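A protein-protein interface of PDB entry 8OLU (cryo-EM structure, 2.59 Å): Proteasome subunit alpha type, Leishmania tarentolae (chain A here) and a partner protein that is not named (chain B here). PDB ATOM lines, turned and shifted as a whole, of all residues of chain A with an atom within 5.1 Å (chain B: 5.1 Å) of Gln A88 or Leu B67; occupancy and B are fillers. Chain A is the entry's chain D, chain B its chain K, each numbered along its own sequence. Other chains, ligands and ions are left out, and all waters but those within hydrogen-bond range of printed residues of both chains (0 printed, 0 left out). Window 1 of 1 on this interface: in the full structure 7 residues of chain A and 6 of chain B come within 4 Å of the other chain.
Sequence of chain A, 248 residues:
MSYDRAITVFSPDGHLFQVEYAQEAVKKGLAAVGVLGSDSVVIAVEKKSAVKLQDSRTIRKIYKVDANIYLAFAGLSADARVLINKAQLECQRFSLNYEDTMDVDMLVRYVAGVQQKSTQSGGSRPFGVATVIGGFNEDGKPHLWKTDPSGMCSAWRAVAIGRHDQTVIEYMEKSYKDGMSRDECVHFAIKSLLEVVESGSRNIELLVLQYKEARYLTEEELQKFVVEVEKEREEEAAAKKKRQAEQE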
ATOM      1  N   LYS A  64      30.037  11.705  25.716  1.00  0.00           N
ATOM      2  CA  LYS A  64      30.401  13.042  25.379  1.00  0.00           C
ATOM      3  C   LYS A  64      29.266  13.912  25.864  1.00  0.00           C
ATOM      4  O   LYS A  64      28.105  13.599  25.651  1.00  0.00           O
ATOM      5  CB  LYS A  64      30.637  13.029  23.884  1.00  0.00           C
ATOM      6  CG  LYS A  64      30.673  14.378  23.224  1.00  0.00           C
ATOM      7  CD  LYS A  64      31.267  14.364  21.881  1.00  0.00           C
ATOM      8  CE  LYS A  64      31.627  15.792  21.542  1.00  0.00           C
ATOM      9  NZ  LYS A  64      31.454  16.087  20.092  1.00  0.00           N
ATOM     10  N   VAL A  65      29.615  14.990  26.542  1.00  0.00           N
ATOM     11  CA  VAL A  65      28.643  15.895  27.101  1.00  0.00           C
ATOM     12  C   VAL A  65      28.602  17.168  26.293  1.00  0.00           C
ATOM     13  O   VAL A  65      27.554  17.768  26.126  1.00  0.00           O
ATOM     14  CB  VAL A  65      29.055  16.195  28.529  1.00  0.00           C
ATOM     15  CG1 VAL A  65      28.216  17.272  29.127  1.00  0.00           C
ATOM     16  CG2 VAL A  65      28.977  14.969  29.386  1.00  0.00           C
ATOM     17  N   LEU A  83      21.107  11.790  33.981  1.00  0.00           N
ATOM     18  CA  LEU A  83      22.063  12.824  34.295  1.00  0.00           C
ATOM     19  C   LEU A  83      22.788  13.373  33.092  1.00  0.00           C
ATOM     20  O   LEU A  83      23.008  14.546  32.989  1.00  0.00           O
ATOM     21  CB  LEU A  83      23.096  12.186  35.177  1.00  0.00           C
ATOM     22  CG  LEU A  83      23.289  12.912  36.477  1.00  0.00           C
ATOM     23  CD1 LEU A  83      21.952  13.319  37.052  1.00  0.00           C
ATOM     24  CD2 LEU A  83      24.046  11.988  37.401  1.00  0.00           C
ATOM     25  N   ILE A  84      23.305  12.502  32.255  1.00  0.00           N
ATOM     26  CA  ILE A  84      24.056  12.882  31.086  1.00  0.00           C
ATOM     27  C   ILE A  84      23.191  13.661  30.137  1.00  0.00           C
ATOM     28  O   ILE A  84      23.689  14.474  29.406  1.00  0.00           O
ATOM     29  CB  ILE A  84      24.564  11.594  30.441  1.00  0.00           C
ATOM     30  CG1 ILE A  84      25.648  11.012  31.324  1.00  0.00           C
ATOM     31  CG2 ILE A  84      25.090  11.800  29.053  1.00  0.00           C
ATOM     32  CD1 ILE A  84      26.085   9.634  30.912  1.00  0.00           C
ATOM     33  N   ASN A  85      21.943  13.276  29.986  1.00  0.00           N
ATOM     34  CA  ASN A  85      21.143  13.977  29.018  1.00  0.00           C
ATOM     35  C   ASN A  85      20.965  15.386  29.561  1.00  0.00           C
ATOM     36  O   ASN A  85      21.115  16.356  28.848  1.00  0.00           O
ATOM     37  CB  ASN A  85      19.872  13.207  28.684  1.00  0.00           C
ATOM     38  CG  ASN A  85      20.062  12.024  27.721  1.00  0.00           C
ATOM     39  OD1 ASN A  85      19.113  11.237  27.586  1.00  0.00           O
ATOM     40  ND2 ASN A  85      21.200  11.864  27.023  1.00  0.00           N
ATOM     41  N   LYS A  86      20.724  15.494  30.862  1.00  0.00           N
ATOM     42  CA  LYS A  86      20.599  16.783  31.483  1.00  0.00           C
ATOM     43  C   LYS A  86      21.860  17.583  31.303  1.00  0.00           C
ATOM     44  O   LYS A  86      21.750  18.769  31.060  1.00  0.00           O
ATOM     45  CB  LYS A  86      20.348  16.631  32.970  1.00  0.00           C
ATOM     46  CG  LYS A  86      18.970  16.103  33.282  1.00  0.00           C
ATOM     47  CD  LYS A  86      18.756  15.928  34.754  1.00  0.00           C
ATOM     48  CE  LYS A  86      17.507  16.642  35.210  1.00  0.00           C
ATOM     49  NZ  LYS A  86      16.718  15.708  36.049  1.00  0.00           N
ATOM     50  N   ALA A  87      23.015  16.958  31.467  1.00  0.00           N
ATOM     51  CA  ALA A  87      24.277  17.647  31.324  1.00  0.00           C
ATOM     52  C   ALA A  87      24.449  18.131  29.895  1.00  0.00           C
ATOM     53  O   ALA A  87      24.815  19.263  29.690  1.00  0.00           O
ATOM     54  CB  ALA A  87      25.422  16.752  31.692  1.00  0.00           C
ATOM     55  N   GLN A  88      24.274  17.253  28.919  1.00  0.00           N
ATOM     56  CA  GLN A  88      24.250  17.624  27.528  1.00  0.00           C
ATOM     57  C   GLN A  88      23.358  18.821  27.315  1.00  0.00           C
ATOM     58  O   GLN A  88      23.709  19.771  26.647  1.00  0.00           O
ATOM     59  CB  GLN A  88      23.752  16.498  26.627  1.00  0.00           C
ATOM     60  CG  GLN A  88      24.808  15.442  26.450  1.00  0.00           C
ATOM     61  CD  GLN A  88      24.303  14.152  25.908  1.00  0.00           C
ATOM     62  OE1 GLN A  88      23.099  13.929  25.911  1.00  0.00           O
ATOM     63  NE2 GLN A  88      25.234  13.278  25.566  1.00  0.00           N
ATOM     64  N   LEU A  89      22.169  18.749  27.834  1.00  0.00           N
ATOM     65  CA  LEU A  89      21.212  19.782  27.499  1.00  0.00           C
ATOM     66  C   LEU A  89      21.649  21.053  28.197  1.00  0.00           C
ATOM     67  O   LEU A  89      21.538  22.101  27.592  1.00  0.00           O
ATOM     68  CB  LEU A  89      19.793  19.305  27.822  1.00  0.00           C
ATOM     69  CG  LEU A  89      18.792  20.405  28.081  1.00  0.00           C
ATOM     70  CD1 LEU A  89      18.722  21.402  26.906  1.00  0.00           C
ATOM     71  CD2 LEU A  89      17.428  19.779  28.331  1.00  0.00           C
ATOM     72  N   GLU A  90      22.276  20.953  29.364  1.00  0.00           N
ATOM     73  CA  GLU A  90      22.757  22.137  30.048  1.00  0.00           C
ATOM     74  C   GLU A  90      23.863  22.840  29.273  1.00  0.00           C
ATOM     75  O   GLU A  90      23.925  24.043  29.241  1.00  0.00           O
ATOM     76  CB  GLU A  90      23.391  21.762  31.377  1.00  0.00           C
ATOM     77  CG  GLU A  90      23.972  22.920  32.122  1.00  0.00           C
ATOM     78  CD  GLU A  90      23.009  24.053  32.472  1.00  0.00           C
ATOM     79  OE1 GLU A  90      23.486  25.066  33.131  1.00  0.00           O
ATOM     80  OE2 GLU A  90      21.771  23.943  32.124  1.00  0.00           O
ATOM     81  N   CYS A  91      24.828  22.103  28.769  1.00  0.00           N
ATOM     82  CA  CYS A  91      25.897  22.710  28.043  1.00  0.00           C
ATOM     83  C   CYS A  91      25.402  23.455  26.831  1.00  0.00           C
ATOM     84  O   CYS A  91      26.008  24.433  26.452  1.00  0.00           O
ATOM     85  CB  CYS A  91      26.801  21.658  27.486  1.00  0.00           C
ATOM     86  SG  CYS A  91      27.833  20.980  28.785  1.00  0.00           S
ATOM     87  N   GLN A  92      24.369  22.948  26.178  1.00  0.00           N
ATOM     88  CA  GLN A  92      23.783  23.686  25.097  1.00  0.00           C
ATOM     89  C   GLN A  92      23.034  24.883  25.650  1.00  0.00           C
ATOM     90  O   GLN A  92      23.113  25.942  25.078  1.00  0.00           O
ATOM     91  CB  GLN A  92      22.910  22.818  24.196  1.00  0.00           C
ATOM     92  CG  GLN A  92      23.740  21.817  23.361  1.00  0.00           C
ATOM     93  CD  GLN A  92      25.051  22.238  22.704  1.00  0.00           C
ATOM     94  OE1 GLN A  92      25.137  23.173  21.898  1.00  0.00           O
ATOM     95  NE2 GLN A  92      26.111  21.515  23.058  1.00  0.00           N
ATOM     96  N   CYS B  63      22.563  24.862  17.956  1.00  0.00           N
ATOM     97  CA  CYS B  63      22.590  24.164  19.220  1.00  0.00           C
ATOM     98  C   CYS B  63      21.835  22.866  19.158  1.00  0.00           C
ATOM     99  O   CYS B  63      22.429  21.813  19.315  1.00  0.00           O
ATOM    100  CB  CYS B  63      21.996  25.031  20.312  1.00  0.00           C
ATOM    101  SG  CYS B  63      23.244  26.308  20.684  1.00  0.00           S
ATOM    102  N   ASN B  64      20.547  22.930  18.862  1.00  0.00           N
ATOM    103  CA  ASN B  64      19.752  21.740  18.689  1.00  0.00           C
ATOM    104  C   ASN B  64      20.353  20.774  17.700  1.00  0.00           C
ATOM    105  O   ASN B  64      20.285  19.596  17.905  1.00  0.00           O
ATOM    106  CB  ASN B  64      18.366  22.093  18.269  1.00  0.00           C
ATOM    107  CG  ASN B  64      17.679  22.605  19.496  1.00  0.00           C
ATOM    108  OD1 ASN B  64      17.387  21.783  20.365  1.00  0.00           O
ATOM    109  ND2 ASN B  64      17.442  23.919  19.590  1.00  0.00           N
ATOM    110  N   LEU B  65      20.972  21.201  16.647  1.00  0.00           N
ATOM    111  CA  LEU B  65      21.601  20.199  15.832  1.00  0.00           C
ATOM    112  C   LEU B  65      22.716  19.530  16.591  1.00  0.00           C
ATOM    113  O   LEU B  65      23.028  18.361  16.288  1.00  0.00           O
ATOM    114  CB  LEU B  65      22.217  20.813  14.586  1.00  0.00           C
ATOM    115  CG  LEU B  65      21.167  21.360  13.644  1.00  0.00           C
ATOM    116  CD1 LEU B  65      21.782  21.649  12.286  1.00  0.00           C
ATOM    117  CD2 LEU B  65      19.973  20.413  13.544  1.00  0.00           C
ATOM    118  N   ALA B  66      23.401  20.339  17.408  1.00  0.00           N
ATOM    119  CA  ALA B  66      24.633  19.882  18.015  1.00  0.00           C
ATOM    120  C   ALA B  66      24.259  18.922  19.129  1.00  0.00           C
ATOM    121  O   ALA B  66      24.803  17.828  19.241  1.00  0.00           O
ATOM    122  CB  ALA B  66      25.474  21.030  18.506  1.00  0.00           C
ATOM    123  N   LEU B  67      23.288  19.366  19.911  1.00  0.00           N
ATOM    124  CA  LEU B  67      22.681  18.529  20.914  1.00  0.00           C
ATOM    125  C   LEU B  67      22.360  17.178  20.318  1.00  0.00           C
ATOM    126  O   LEU B  67      22.792  16.199  20.872  1.00  0.00           O
ATOM    127  CB  LEU B  67      21.399  19.191  21.390  1.00  0.00           C
ATOM    128  CG  LEU B  67      20.727  18.476  22.552  1.00  0.00           C
ATOM    129  CD1 LEU B  67      21.779  18.113  23.570  1.00  0.00           C
ATOM    130  CD2 LEU B  67      19.656  19.375  23.184  1.00  0.00           C
ATOM    131  N   ASN B  68      21.629  17.154  19.207  1.00  0.00           N
ATOM    132  CA  ASN B  68      21.095  15.938  18.644  1.00  0.00           C
ATOM    133  C   ASN B  68      22.233  15.082  18.139  1.00  0.00           C
ATOM    134  O   ASN B  68      22.118  13.898  18.096  1.00  0.00           O
ATOM    135  CB  ASN B  68      20.161  16.152  17.456  1.00  0.00           C
ATOM    136  CG  ASN B  68      18.897  16.941  17.760  1.00  0.00           C
ATOM    137  OD1 ASN B  68      18.600  17.286  18.904  1.00  0.00           O
ATOM    138  ND2 ASN B  68      18.181  17.331  16.709  1.00  0.00           N
ATOM    139  N   ARG B  69      23.316  15.659  17.712  1.00  0.00           N
ATOM    140  CA  ARG B  69      24.447  14.908  17.215  1.00  0.00           C
ATOM    141  C   ARG B  69      25.192  14.268  18.401  1.00  0.00           C
ATOM    142  O   ARG B  69      25.880  13.259  18.209  1.00  0.00           O
ATOM    143  CB  ARG B  69      25.250  15.908  16.377  1.00  0.00           C
ATOM    144  CG  ARG B  69      26.429  15.361  15.598  1.00  0.00           C
ATOM    145  CD  ARG B  69      27.247  16.401  14.848  1.00  0.00           C
ATOM    146  NE  ARG B  69      27.662  17.507  15.727  1.00  0.00           N
ATOM    147  CZ  ARG B  69      27.223  18.773  15.660  1.00  0.00           C
ATOM    148  NH1 ARG B  69      27.827  19.703  16.382  1.00  0.00           N
ATOM    149  NH2 ARG B  69      26.198  19.104  14.881  1.00  0.00           N
ATOM    150  N   MET B  70      25.110  14.860  19.607  1.00  0.00           N
ATOM    151  CA  MET B  70      25.684  14.260  20.807  1.00  0.00           C
ATOM    152  C   MET B  70      24.847  13.029  21.051  1.00  0.00           C
ATOM    153  O   MET B  70      25.390  11.930  21.068  1.00  0.00           O
ATOM    154  CB  MET B  70      25.441  14.968  22.156  1.00  0.00           C
ATOM    155  CG  MET B  70      25.985  16.313  22.417  1.00  0.00           C
ATOM    156  SD  MET B  70      27.678  16.100  22.642  1.00  0.00           S
ATOM    157  CE  MET B  70      28.277  16.949  21.172  1.00  0.00           C
ATOM    158  N   ARG B  71      23.535  13.289  21.311  1.00  0.00           N
ATOM    159  CA  ARG B  71      22.555  12.298  21.739  1.00  0.00           C
ATOM    160  C   ARG B  71      22.348  11.298  20.595  1.00  0.00           C
ATOM    161  O   ARG B  71      21.345  10.600  20.558  1.00  0.00           O
ATOM    162  CB  ARG B  71      21.218  12.903  22.186  1.00  0.00           C
ATOM    163  CG  ARG B  71      21.340  14.108  23.103  1.00  0.00           C
ATOM    164  CD  ARG B  71      20.334  14.298  24.253  1.00  0.00           C
ATOM    165  NE  ARG B  71      19.072  14.875  23.823  1.00  0.00           N
ATOM    166  CZ  ARG B  71      18.475  15.893  24.445  1.00  0.00           C
ATOM    167  NH1 ARG B  71      17.528  16.605  23.836  1.00  0.00           N
ATOM    168  NH2 ARG B  71      18.879  16.213  25.670  1.00  0.00           N
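O of Lys A64 is in hydrogen-bond range of NE2 of Gln A88 (2.9 Å). ND2 of Asn A85 sits at hydrogen-bond distance from OE1 of Gln A88 (3.0 Å).
Lys A64 touches Met B70. Val A65 touches Met B70. CD of Arg B71 touches ND2 of Asn A85, 3.8 Å away. Leu B67 touches Gln A88 (CD1 to CB, 3.98 Å). Gln A88 touches Met B70. Gln A88 touches Arg B71 (OE1 to CD, 3.2 Å). Arg B71 touches Leu A89 (NH2 to CB, 3.9 Å). Gln A92 touches Cys B63 (OE1 to CA, 3.8 Å).
Of the printed residues of chain B, Lys A64 touches Met B70. Of the printed residues of chain B, Val A65 touches Met B70. Of the printed residues of chain B, Asn A85 touches Arg B71 (3.8 Å). Lys A86 touches none of the printed residues of chain B. Printed residues of chain B within 4 Å of Gln A88: Leu B67, Met B70 and Arg B71. Glu A90 touches none of the printed residues of chain B. Printed residues of chain A within 4 Å of Cys B63: Gln A92. Of the printed residues of chain A, Arg B71 touches Asn A85 (3.8 Å), Gln A88 (3.2 Å) and Leu A89 (3.9 Å). The nearest printed residue of chain A that does not touch Leu B67 is Gln A92 (4.03 Å). The nearest printed residue of chain A that does not touch Met B70 is Gln A92 (5.2 Å).
Printed residues of chain A that touch a printed residue of chain B: Lys A64, Val A65, Asn A85, Gln A88, Leu A89 and Gln A92. Hydrophobic or aromatic side chains of chain B that line the printed part of chain A: Leu B67 and Met B70. Among the printed residues, no Asp or Glu carboxylate lies within 4 Å of a Lys or Arg side-chain nitrogen of the other chain.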
